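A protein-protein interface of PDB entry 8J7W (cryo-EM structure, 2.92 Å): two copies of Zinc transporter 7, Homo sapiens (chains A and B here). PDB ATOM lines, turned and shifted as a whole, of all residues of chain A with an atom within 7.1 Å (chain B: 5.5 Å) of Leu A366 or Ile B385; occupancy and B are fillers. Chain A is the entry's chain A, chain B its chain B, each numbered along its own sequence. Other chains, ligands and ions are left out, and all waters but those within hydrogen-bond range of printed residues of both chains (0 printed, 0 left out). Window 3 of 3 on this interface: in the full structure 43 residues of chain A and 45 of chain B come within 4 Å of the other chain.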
ATOM      1  N   LEU A 329      33.433  14.917   1.014  1.00  0.00           N
ATOM      2  CA  LEU A 329      32.661  16.152   1.017  1.00  0.00           C
ATOM      3  C   LEU A 329      33.560  17.346   0.731  1.00  0.00           C
ATOM      4  O   LEU A 329      34.720  17.386   1.148  1.00  0.00           O
ATOM      5  CB  LEU A 329      31.958  16.334   2.359  1.00  0.00           C
ATOM      6  CG  LEU A 329      30.719  15.477   2.613  1.00  0.00           C
ATOM      7  CD1 LEU A 329      30.105  15.824   3.955  1.00  0.00           C
ATOM      8  CD2 LEU A 329      29.713  15.651   1.492  1.00  0.00           C
ATOM      9  N   LEU A 354      34.863  17.003  12.772  1.00  0.00           N
ATOM     10  CA  LEU A 354      35.293  17.309  11.415  1.00  0.00           C
ATOM     11  C   LEU A 354      36.208  18.523  11.425  1.00  0.00           C
ATOM     12  O   LEU A 354      35.850  19.570  11.973  1.00  0.00           O
ATOM     13  CB  LEU A 354      34.096  17.574  10.502  1.00  0.00           C
ATOM     14  CG  LEU A 354      33.270  16.374  10.050  1.00  0.00           C
ATOM     15  CD1 LEU A 354      32.216  16.806   9.057  1.00  0.00           C
ATOM     16  CD2 LEU A 354      34.169  15.332   9.439  1.00  0.00           C
ATOM     17  N   ASP A 361      31.654  25.564   3.812  1.00  0.00           N
ATOM     18  CA  ASP A 361      30.213  25.649   4.033  1.00  0.00           C
ATOM     19  C   ASP A 361      29.836  24.696   5.159  1.00  0.00           C
ATOM     20  O   ASP A 361      29.639  23.501   4.936  1.00  0.00           O
ATOM     21  CB  ASP A 361      29.463  25.318   2.748  1.00  0.00           C
ATOM     22  CG  ASP A 361      28.024  25.793   2.766  1.00  0.00           C
ATOM     23  OD1 ASP A 361      27.581  26.357   3.785  1.00  0.00           O
ATOM     24  OD2 ASP A 361      27.329  25.604   1.748  1.00  0.00           O
ATOM     25  N   ALA A 362      29.736  25.226   6.379  1.00  0.00           N
ATOM     26  CA  ALA A 362      29.464  24.380   7.536  1.00  0.00           C
ATOM     27  C   ALA A 362      28.030  23.864   7.530  1.00  0.00           C
ATOM     28  O   ALA A 362      27.774  22.735   7.963  1.00  0.00           O
ATOM     29  CB  ALA A 362      29.754  25.147   8.825  1.00  0.00           C
ATOM     30  N   ARG A 363      27.085  24.674   7.045  1.00  0.00           N
ATOM     31  CA  ARG A 363      25.692  24.245   6.974  1.00  0.00           C
ATOM     32  C   ARG A 363      25.542  23.038   6.056  1.00  0.00           C
ATOM     33  O   ARG A 363      24.943  22.020   6.431  1.00  0.00           O
ATOM     34  CB  ARG A 363      24.819  25.394   6.471  1.00  0.00           C
ATOM     35  CG  ARG A 363      24.490  26.466   7.491  1.00  0.00           C
ATOM     36  CD  ARG A 363      24.114  27.752   6.776  1.00  0.00           C
ATOM     37  NE  ARG A 363      23.946  28.884   7.677  1.00  0.00           N
ATOM     38  CZ  ARG A 363      24.819  29.872   7.810  1.00  0.00           C
ATOM     39  NH1 ARG A 363      25.952  29.888   7.131  1.00  0.00           N
ATOM     40  NH2 ARG A 363      24.549  30.870   8.645  1.00  0.00           N
ATOM     41  N   TRP A 364      26.097  23.139   4.848  1.00  0.00           N
ATOM     42  CA  TRP A 364      25.990  22.060   3.876  1.00  0.00           C
ATOM     43  C   TRP A 364      26.741  20.820   4.336  1.00  0.00           C
ATOM     44  O   TRP A 364      26.256  19.698   4.165  1.00  0.00           O
ATOM     45  CB  TRP A 364      26.509  22.531   2.520  1.00  0.00           C
ATOM     46  CG  TRP A 364      26.544  21.455   1.496  1.00  0.00           C
ATOM     47  CD1 TRP A 364      25.491  20.964   0.790  1.00  0.00           C
ATOM     48  CD2 TRP A 364      27.692  20.714   1.074  1.00  0.00           C
ATOM     49  NE1 TRP A 364      25.910  19.969  -0.053  1.00  0.00           N
ATOM     50  CE2 TRP A 364      27.259  19.797   0.100  1.00  0.00           C
ATOM     51  CE3 TRP A 364      29.046  20.743   1.419  1.00  0.00           C
ATOM     52  CZ2 TRP A 364      28.129  18.913  -0.530  1.00  0.00           C
ATOM     53  CZ3 TRP A 364      29.906  19.867   0.795  1.00  0.00           C
ATOM     54  CH2 TRP A 364      29.446  18.964  -0.169  1.00  0.00           C
ATOM     55  N   ILE A 365      27.933  21.000   4.909  1.00  0.00           N
ATOM     56  CA  ILE A 365      28.718  19.859   5.373  1.00  0.00           C
ATOM     57  C   ILE A 365      27.994  19.142   6.506  1.00  0.00           C
ATOM     58  O   ILE A 365      27.958  17.906   6.555  1.00  0.00           O
ATOM     59  CB  ILE A 365      30.130  20.319   5.783  1.00  0.00           C
ATOM     60  CG1 ILE A 365      31.005  20.504   4.542  1.00  0.00           C
ATOM     61  CG2 ILE A 365      30.780  19.332   6.736  1.00  0.00           C
ATOM     62  CD1 ILE A 365      32.302  21.217   4.807  1.00  0.00           C
ATOM     63  N   LEU A 366      27.387  19.904   7.418  1.00  0.00           N
ATOM     64  CA  LEU A 366      26.608  19.304   8.496  1.00  0.00           C
ATOM     65  C   LEU A 366      25.421  18.519   7.948  1.00  0.00           C
ATOM     66  O   LEU A 366      25.171  17.379   8.360  1.00  0.00           O
ATOM     67  CB  LEU A 366      26.135  20.392   9.460  1.00  0.00           C
ATOM     68  CG  LEU A 366      25.568  19.940  10.806  1.00  0.00           C
ATOM     69  CD1 LEU A 366      26.644  19.296  11.648  1.00  0.00           C
ATOM     70  CD2 LEU A 366      24.947  21.109  11.541  1.00  0.00           C
ATOM     71  N   SER A 367      24.687  19.114   7.003  1.00  0.00           N
ATOM     72  CA  SER A 367      23.528  18.433   6.434  1.00  0.00           C
ATOM     73  C   SER A 367      23.933  17.166   5.688  1.00  0.00           C
ATOM     74  O   SER A 367      23.258  16.134   5.787  1.00  0.00           O
ATOM     75  CB  SER A 367      22.763  19.383   5.513  1.00  0.00           C
ATOM     76  OG  SER A 367      23.469  19.607   4.307  1.00  0.00           O
ATOM     77  N   GLN A 368      25.048  17.213   4.959  1.00  0.00           N
ATOM     78  CA  GLN A 368      25.484  16.048   4.199  1.00  0.00           C
ATOM     79  C   GLN A 368      25.993  14.941   5.110  1.00  0.00           C
ATOM     80  O   GLN A 368      25.730  13.760   4.860  1.00  0.00           O
ATOM     81  CB  GLN A 368      26.558  16.447   3.191  1.00  0.00           C
ATOM     82  CG  GLN A 368      26.058  17.319   2.064  1.00  0.00           C
ATOM     83  CD  GLN A 368      25.029  16.632   1.197  1.00  0.00           C
ATOM     84  OE1 GLN A 368      23.870  17.036   1.154  1.00  0.00           O
ATOM     85  NE2 GLN A 368      25.448  15.589   0.495  1.00  0.00           N
ATOM     86  N   THR A 369      26.736  15.295   6.164  1.00  0.00           N
ATOM     87  CA  THR A 369      27.192  14.287   7.117  1.00  0.00           C
ATOM     88  C   THR A 369      26.013  13.627   7.817  1.00  0.00           C
ATOM     89  O   THR A 369      25.989  12.399   7.995  1.00  0.00           O
ATOM     90  CB  THR A 369      28.140  14.920   8.136  1.00  0.00           C
ATOM     91  OG1 THR A 369      29.161  15.653   7.451  1.00  0.00           O
ATOM     92  CG2 THR A 369      28.792  13.858   9.000  1.00  0.00           C
ATOM     93  N   HIS A 370      25.015  14.426   8.206  1.00  0.00           N
ATOM     94  CA  HIS A 370      23.826  13.864   8.833  1.00  0.00           C
ATOM     95  C   HIS A 370      23.070  12.956   7.875  1.00  0.00           C
ATOM     96  O   HIS A 370      22.586  11.895   8.278  1.00  0.00           O
ATOM     97  CB  HIS A 370      22.928  14.980   9.350  1.00  0.00           C
ATOM     98  CG  HIS A 370      23.094  15.251  10.810  1.00  0.00           C
ATOM     99  ND1 HIS A 370      23.943  16.220  11.296  1.00  0.00           N
ATOM    100  CD2 HIS A 370      22.534  14.663  11.892  1.00  0.00           C
ATOM    101  CE1 HIS A 370      23.893  16.222  12.615  1.00  0.00           C
ATOM    102  NE2 HIS A 370      23.045  15.288  13.002  1.00  0.00           N
ATOM    103  N   ASN A 371      22.970  13.342   6.601  1.00  0.00           N
ATOM    104  CA  ASN A 371      22.347  12.463   5.616  1.00  0.00           C
ATOM    105  C   ASN A 371      23.106  11.147   5.487  1.00  0.00           C
ATOM    106  O   ASN A 371      22.503  10.068   5.547  1.00  0.00           O
ATOM    107  CB  ASN A 371      22.268  13.162   4.260  1.00  0.00           C
ATOM    108  CG  ASN A 371      21.215  14.243   4.222  1.00  0.00           C
ATOM    109  OD1 ASN A 371      20.109  14.064   4.727  1.00  0.00           O
ATOM    110  ND2 ASN A 371      21.549  15.373   3.613  1.00  0.00           N
ATOM    111  N   ILE A 372      24.432  11.224   5.342  1.00  0.00           N
ATOM    112  CA  ILE A 372      25.255  10.036   5.128  1.00  0.00           C
ATOM    113  C   ILE A 372      25.106   9.062   6.287  1.00  0.00           C
ATOM    114  O   ILE A 372      24.954   7.852   6.085  1.00  0.00           O
ATOM    115  CB  ILE A 372      26.728  10.439   4.916  1.00  0.00           C
ATOM    116  CG1 ILE A 372      26.929  11.048   3.531  1.00  0.00           C
ATOM    117  CG2 ILE A 372      27.655   9.248   5.108  1.00  0.00           C
ATOM    118  CD1 ILE A 372      28.136  11.943   3.435  1.00  0.00           C
ATOM    119  N   LEU A 381      23.098  11.556  16.006  1.00  0.00           N
ATOM    120  CA  LEU A 381      24.391  11.921  15.448  1.00  0.00           C
ATOM    121  C   LEU A 381      24.789  13.307  15.926  1.00  0.00           C
ATOM    122  O   LEU A 381      23.983  14.240  15.884  1.00  0.00           O
ATOM    123  CB  LEU A 381      24.371  11.876  13.920  1.00  0.00           C
ATOM    124  CG  LEU A 381      25.733  12.051  13.253  1.00  0.00           C
ATOM    125  CD1 LEU A 381      26.582  10.808  13.433  1.00  0.00           C
ATOM    126  CD2 LEU A 381      25.549  12.369  11.785  1.00  0.00           C
ATOM    127  N   TYR A 382      26.033  13.434  16.377  1.00  0.00           N
ATOM    128  CA  TYR A 382      26.616  14.711  16.764  1.00  0.00           C
ATOM    129  C   TYR A 382      27.858  14.939  15.919  1.00  0.00           C
ATOM    130  O   TYR A 382      28.820  14.169  16.006  1.00  0.00           O
ATOM    131  CB  TYR A 382      26.967  14.733  18.252  1.00  0.00           C
ATOM    132  CG  TYR A 382      25.764  14.760  19.160  1.00  0.00           C
ATOM    133  CD1 TYR A 382      25.103  13.590  19.505  1.00  0.00           C
ATOM    134  CD2 TYR A 382      25.285  15.957  19.664  1.00  0.00           C
ATOM    135  CE1 TYR A 382      24.001  13.616  20.331  1.00  0.00           C
ATOM    136  CE2 TYR A 382      24.186  15.991  20.490  1.00  0.00           C
ATOM    137  CZ  TYR A 382      23.548  14.821  20.820  1.00  0.00           C
ATOM    138  OH  TYR A 382      22.453  14.864  21.646  1.00  0.00           O
ATOM    139  N   VAL A 383      27.836  15.987  15.103  1.00  0.00           N
ATOM    140  CA  VAL A 383      28.960  16.340  14.247  1.00  0.00           C
ATOM    141  C   VAL A 383      29.493  17.683  14.710  1.00  0.00           C
ATOM    142  O   VAL A 383      28.845  18.718  14.515  1.00  0.00           O
ATOM    143  CB  VAL A 383      28.569  16.392  12.766  1.00  0.00           C
ATOM    144  CG1 VAL A 383      29.811  16.491  11.902  1.00  0.00           C
ATOM    145  CG2 VAL A 383      27.751  15.177  12.393  1.00  0.00           C
ATOM    146  N   GLN A 384      30.674  17.672  15.317  1.00  0.00           N
ATOM    147  CA  GLN A 384      31.384  18.896  15.646  1.00  0.00           C
ATOM    148  C   GLN A 384      32.256  19.287  14.461  1.00  0.00           C
ATOM    149  O   GLN A 384      33.024  18.465  13.951  1.00  0.00           O
ATOM    150  CB  GLN A 384      32.231  18.720  16.903  1.00  0.00           C
ATOM    151  CG  GLN A 384      33.001  19.962  17.286  1.00  0.00           C
ATOM    152  CD  GLN A 384      33.680  19.821  18.620  1.00  0.00           C
ATOM    153  OE1 GLN A 384      33.060  19.415  19.597  1.00  0.00           O
ATOM    154  NE2 GLN A 384      34.958  20.162  18.675  1.00  0.00           N
ATOM    155  N   ILE A 385      32.134  20.533  14.023  1.00  0.00           N
ATOM    156  CA  ILE A 385      32.868  21.047  12.875  1.00  0.00           C
ATOM    157  C   ILE A 385      33.876  22.066  13.384  1.00  0.00           C
ATOM    158  O   ILE A 385      33.501  23.048  14.036  1.00  0.00           O
ATOM    159  CB  ILE A 385      31.921  21.662  11.834  1.00  0.00           C
ATOM    160  CG1 ILE A 385      31.158  20.558  11.101  1.00  0.00           C
ATOM    161  CG2 ILE A 385      32.682  22.537  10.860  1.00  0.00           C
ATOM    162  CD1 ILE A 385      30.092  21.067  10.176  1.00  0.00           C
ATOM    163  N   LYS B 353      23.847  20.059  21.254  1.00  0.00           N
ATOM    164  CA  LYS B 353      23.672  20.781  20.004  1.00  0.00           C
ATOM    165  C   LYS B 353      23.301  22.223  20.307  1.00  0.00           C
ATOM    166  O   LYS B 353      22.406  22.482  21.116  1.00  0.00           O
ATOM    167  CB  LYS B 353      22.608  20.119  19.128  1.00  0.00           C
ATOM    168  CG  LYS B 353      23.038  18.765  18.605  1.00  0.00           C
ATOM    169  CD  LYS B 353      21.986  18.121  17.736  1.00  0.00           C
ATOM    170  CE  LYS B 353      22.438  16.742  17.296  1.00  0.00           C
ATOM    171  NZ  LYS B 353      21.350  15.974  16.643  1.00  0.00           N
ATOM    172  N   LEU B 354      23.993  23.154  19.662  1.00  0.00           N
ATOM    173  CA  LEU B 354      23.759  24.577  19.838  1.00  0.00           C
ATOM    174  C   LEU B 354      23.107  25.156  18.594  1.00  0.00           C
ATOM    175  O   LEU B 354      23.591  24.961  17.477  1.00  0.00           O
ATOM    176  CB  LEU B 354      25.062  25.327  20.120  1.00  0.00           C
ATOM    177  CG  LEU B 354      25.789  25.020  21.425  1.00  0.00           C
ATOM    178  CD1 LEU B 354      26.958  25.959  21.600  1.00  0.00           C
ATOM    179  CD2 LEU B 354      24.839  25.140  22.588  1.00  0.00           C
ATOM    180  N   VAL B 356      22.577  28.664  16.962  1.00  0.00           N
ATOM    181  CA  VAL B 356      23.217  29.964  17.115  1.00  0.00           C
ATOM    182  C   VAL B 356      22.660  30.938  16.090  1.00  0.00           C
ATOM    183  O   VAL B 356      21.779  30.590  15.297  1.00  0.00           O
ATOM    184  CB  VAL B 356      24.749  29.852  16.999  1.00  0.00           C
ATOM    185  CG1 VAL B 356      25.306  28.957  18.099  1.00  0.00           C
ATOM    186  CG2 VAL B 356      25.147  29.341  15.629  1.00  0.00           C
ATOM    187  N   ALA B 362      31.273  30.927  15.290  1.00  0.00           N
ATOM    188  CA  ALA B 362      31.248  29.505  15.623  1.00  0.00           C
ATOM    189  C   ALA B 362      32.540  29.066  16.298  1.00  0.00           C
ATOM    190  O   ALA B 362      32.519  28.216  17.195  1.00  0.00           O
ATOM    191  CB  ALA B 362      30.992  28.676  14.365  1.00  0.00           C
ATOM    192  N   ILE B 365      32.395  30.403  19.940  1.00  0.00           N
ATOM    193  CA  ILE B 365      31.358  29.698  20.689  1.00  0.00           C
ATOM    194  C   ILE B 365      31.802  28.273  20.995  1.00  0.00           C
ATOM    195  O   ILE B 365      31.593  27.765  22.104  1.00  0.00           O
ATOM    196  CB  ILE B 365      30.027  29.735  19.918  1.00  0.00           C
ATOM    197  CG1 ILE B 365      29.371  31.111  20.049  1.00  0.00           C
ATOM    198  CG2 ILE B 365      29.078  28.665  20.410  1.00  0.00           C
ATOM    199  CD1 ILE B 365      28.215  31.331  19.107  1.00  0.00           C
ATOM    200  N   LEU B 366      32.440  27.614  20.026  1.00  0.00           N
ATOM    201  CA  LEU B 366      32.950  26.264  20.246  1.00  0.00           C
ATOM    202  C   LEU B 366      34.015  26.251  21.334  1.00  0.00           C
ATOM    203  O   LEU B 366      33.980  25.412  22.244  1.00  0.00           O
ATOM    204  CB  LEU B 366      33.506  25.706  18.937  1.00  0.00           C
ATOM    205  CG  LEU B 366      33.752  24.201  18.841  1.00  0.00           C
ATOM    206  CD1 LEU B 366      32.476  23.438  19.092  1.00  0.00           C
ATOM    207  CD2 LEU B 366      34.311  23.857  17.483  1.00  0.00           C
ATOM    208  N   VAL B 383      30.269  19.274  20.569  1.00  0.00           N
ATOM    209  CA  VAL B 383      29.343  20.388  20.426  1.00  0.00           C
ATOM    210  C   VAL B 383      29.014  20.544  18.951  1.00  0.00           C
ATOM    211  O   VAL B 383      29.875  20.927  18.150  1.00  0.00           O
ATOM    212  CB  VAL B 383      29.921  21.690  20.997  1.00  0.00           C
ATOM    213  CG1 VAL B 383      28.824  22.729  21.143  1.00  0.00           C
ATOM    214  CG2 VAL B 383      30.598  21.429  22.324  1.00  0.00           C
ATOM    215  N   GLN B 384      27.771  20.249  18.593  1.00  0.00           N
ATOM    216  CA  GLN B 384      27.262  20.515  17.258  1.00  0.00           C
ATOM    217  C   GLN B 384      26.651  21.908  17.235  1.00  0.00           C
ATOM    218  O   GLN B 384      25.855  22.257  18.109  1.00  0.00           O
ATOM    219  CB  GLN B 384      26.227  19.472  16.843  1.00  0.00           C
ATOM    220  CG  GLN B 384      25.718  19.656  15.430  1.00  0.00           C
ATOM    221  CD  GLN B 384      24.788  18.552  15.007  1.00  0.00           C
ATOM    222  OE1 GLN B 384      25.135  17.378  15.083  1.00  0.00           O
ATOM    223  NE2 GLN B 384      23.598  18.919  14.554  1.00  0.00           N
ATOM    224  N   ILE B 385      27.036  22.703  16.246  1.00  0.00           N
ATOM    225  CA  ILE B 385      26.573  24.076  16.116  1.00  0.00           C
ATOM    226  C   ILE B 385      25.693  24.155  14.878  1.00  0.00           C
ATOM    227  O   ILE B 385      26.114  23.766  13.782  1.00  0.00           O
ATOM    228  CB  ILE B 385      27.748  25.060  16.039  1.00  0.00           C
ATOM    229  CG1 ILE B 385      28.318  25.301  17.437  1.00  0.00           C
ATOM    230  CG2 ILE B 385      27.320  26.367  15.395  1.00  0.00           C
ATOM    231  CD1 ILE B 385      29.637  26.018  17.444  1.00  0.00           C
ATOM    232  N   ASP B 386      24.470  24.638  15.058  1.00  0.00           N
ATOM    233  CA  ASP B 386      23.529  24.841  13.967  1.00  0.00           C
ATOM    234  C   ASP B 386      23.260  26.330  13.818  1.00  0.00           C
ATOM    235  O   ASP B 386      22.937  27.008  14.797  1.00  0.00           O
ATOM    236  CB  ASP B 386      22.221  24.087  14.215  1.00  0.00           C
ATOM    237  CG  ASP B 386      22.443  22.703  14.796  1.00  0.00           C
ATOM    238  OD1 ASP B 386      22.906  21.813  14.052  1.00  0.00           O
ATOM    239  OD2 ASP B 386      22.153  22.502  15.995  1.00  0.00           O
ATOM    240  N   PHE B 387      23.396  26.833  12.596  1.00  0.00           N
ATOM    241  CA  PHE B 387      23.098  28.229  12.313  1.00  0.00           C
ATOM    242  C   PHE B 387      21.611  28.375  12.027  1.00  0.00           C
ATOM    243  O   PHE B 387      21.076  27.698  11.145  1.00  0.00           O
ATOM    244  CB  PHE B 387      23.926  28.720  11.131  1.00  0.00           C
ATOM    245  CG  PHE B 387      25.396  28.762  11.399  1.00  0.00           C
ATOM    246  CD1 PHE B 387      25.963  29.836  12.062  1.00  0.00           C
ATOM    247  CD2 PHE B 387      26.216  27.725  10.990  1.00  0.00           C
ATOM    248  CE1 PHE B 387      27.317  29.874  12.312  1.00  0.00           C
ATOM    249  CE2 PHE B 387      27.571  27.759  11.238  1.00  0.00           C
ATOM    250  CZ  PHE B 387      28.122  28.834  11.901  1.00  0.00           C
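The backbone carbonyl oxygen (O) of Leu A381 sits at hydrogen-bond distance from the side-chain amino group (NZ) of Lys B353 (3.2 Å).
The backbone carbonyl oxygen (O) of Leu A381 sits close to the side-chain amide oxygen (OE1) of Gln B384 (3.4 Å).
The side-chain amide oxygen (OE1) of Gln B384 lies within hydrogen-bond range of the backbone NH (N) of Val A383 (3.0 Å).
The backbone NH of Val B383 lies within hydrogen-bond range of the side-chain amide oxygen of Gln A384, 3.0 Å away.
The backbone NH (N) of Leu A354 sits at hydrogen-bond distance from the backbone carbonyl oxygen (O) of Gln A384 (2.6 Å).
O of Leu A366 sits at hydrogen-bond distance from ND1 of His A370 (3.4 Å).
A ring nitrogen (NE2) of His A370 is in hydrogen-bond range of the backbone carbonyl oxygen (O) of Leu A381 (3.2 Å).
O of Leu B354 is in hydrogen-bond range of N of Asp B386 (2.6 Å).
O of Asp B386 sits at hydrogen-bond distance from N of Val B356 (2.7 Å).
The side-chain amide nitrogen (NE2) of Gln B384 sits at hydrogen-bond distance from the side-chain carboxylate (OD1) of Asp B386.
Phe B387 touches Arg A363.
Gln B384 touches Leu A366 (CD to CD1, 3.9 Å).
CD2 of Leu A366 touches O of Ile B385, at 3.7 Å.
Leu A366 touches Asp B386.
Gln B384 touches His A370 (OE1 to CE1, 3.0 Å).
Tyr A382 touches Lys B353 (CE2 to CG, 3.5 Å).
CA of Tyr A382 touches OE1 of Gln B384, 3.5 Å away.
Leu B366 touches Gln A384 (CD1 to CD, 3.8 Å).
Leu B366 touches Ile A385.
Leu A366 touches three residues of chain B.
Of the printed residues of chain B, Val A383 touches Gln B384.
Of the printed residues of chain A, Val B383 touches Gln A384 (3.0 Å).
Printed residues of chain A within 4 Å of Phe B387: Arg A363.
Printed residues of chain A within 4 Å of Asp B386: Leu A366 (3.3 Å).
Thr A369 touches none of the printed residues of chain B.
Ile B365 touches none of the printed residues of chain A.
The nearest residue of chain A that does not touch Ile B385 is Val A383 (4.7 Å).
The nearest printed residue of chain B that does not touch Val A383 is Val B383 (4.4 Å).
Among the printed residues, no Asp or Glu carboxylate lies within 4 Å of a Lys or Arg side-chain nitrogen of the other chain.
Leu A366 touches Gln B384, and with the chains exchanged Gln A384 touches Leu B366.
Leu A366 touches Ile B385, and with the chains exchanged Ile A385 touches Leu B366.
Val A383 touches Gln B384, and with the chains exchanged Gln A384 touches Val B383.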
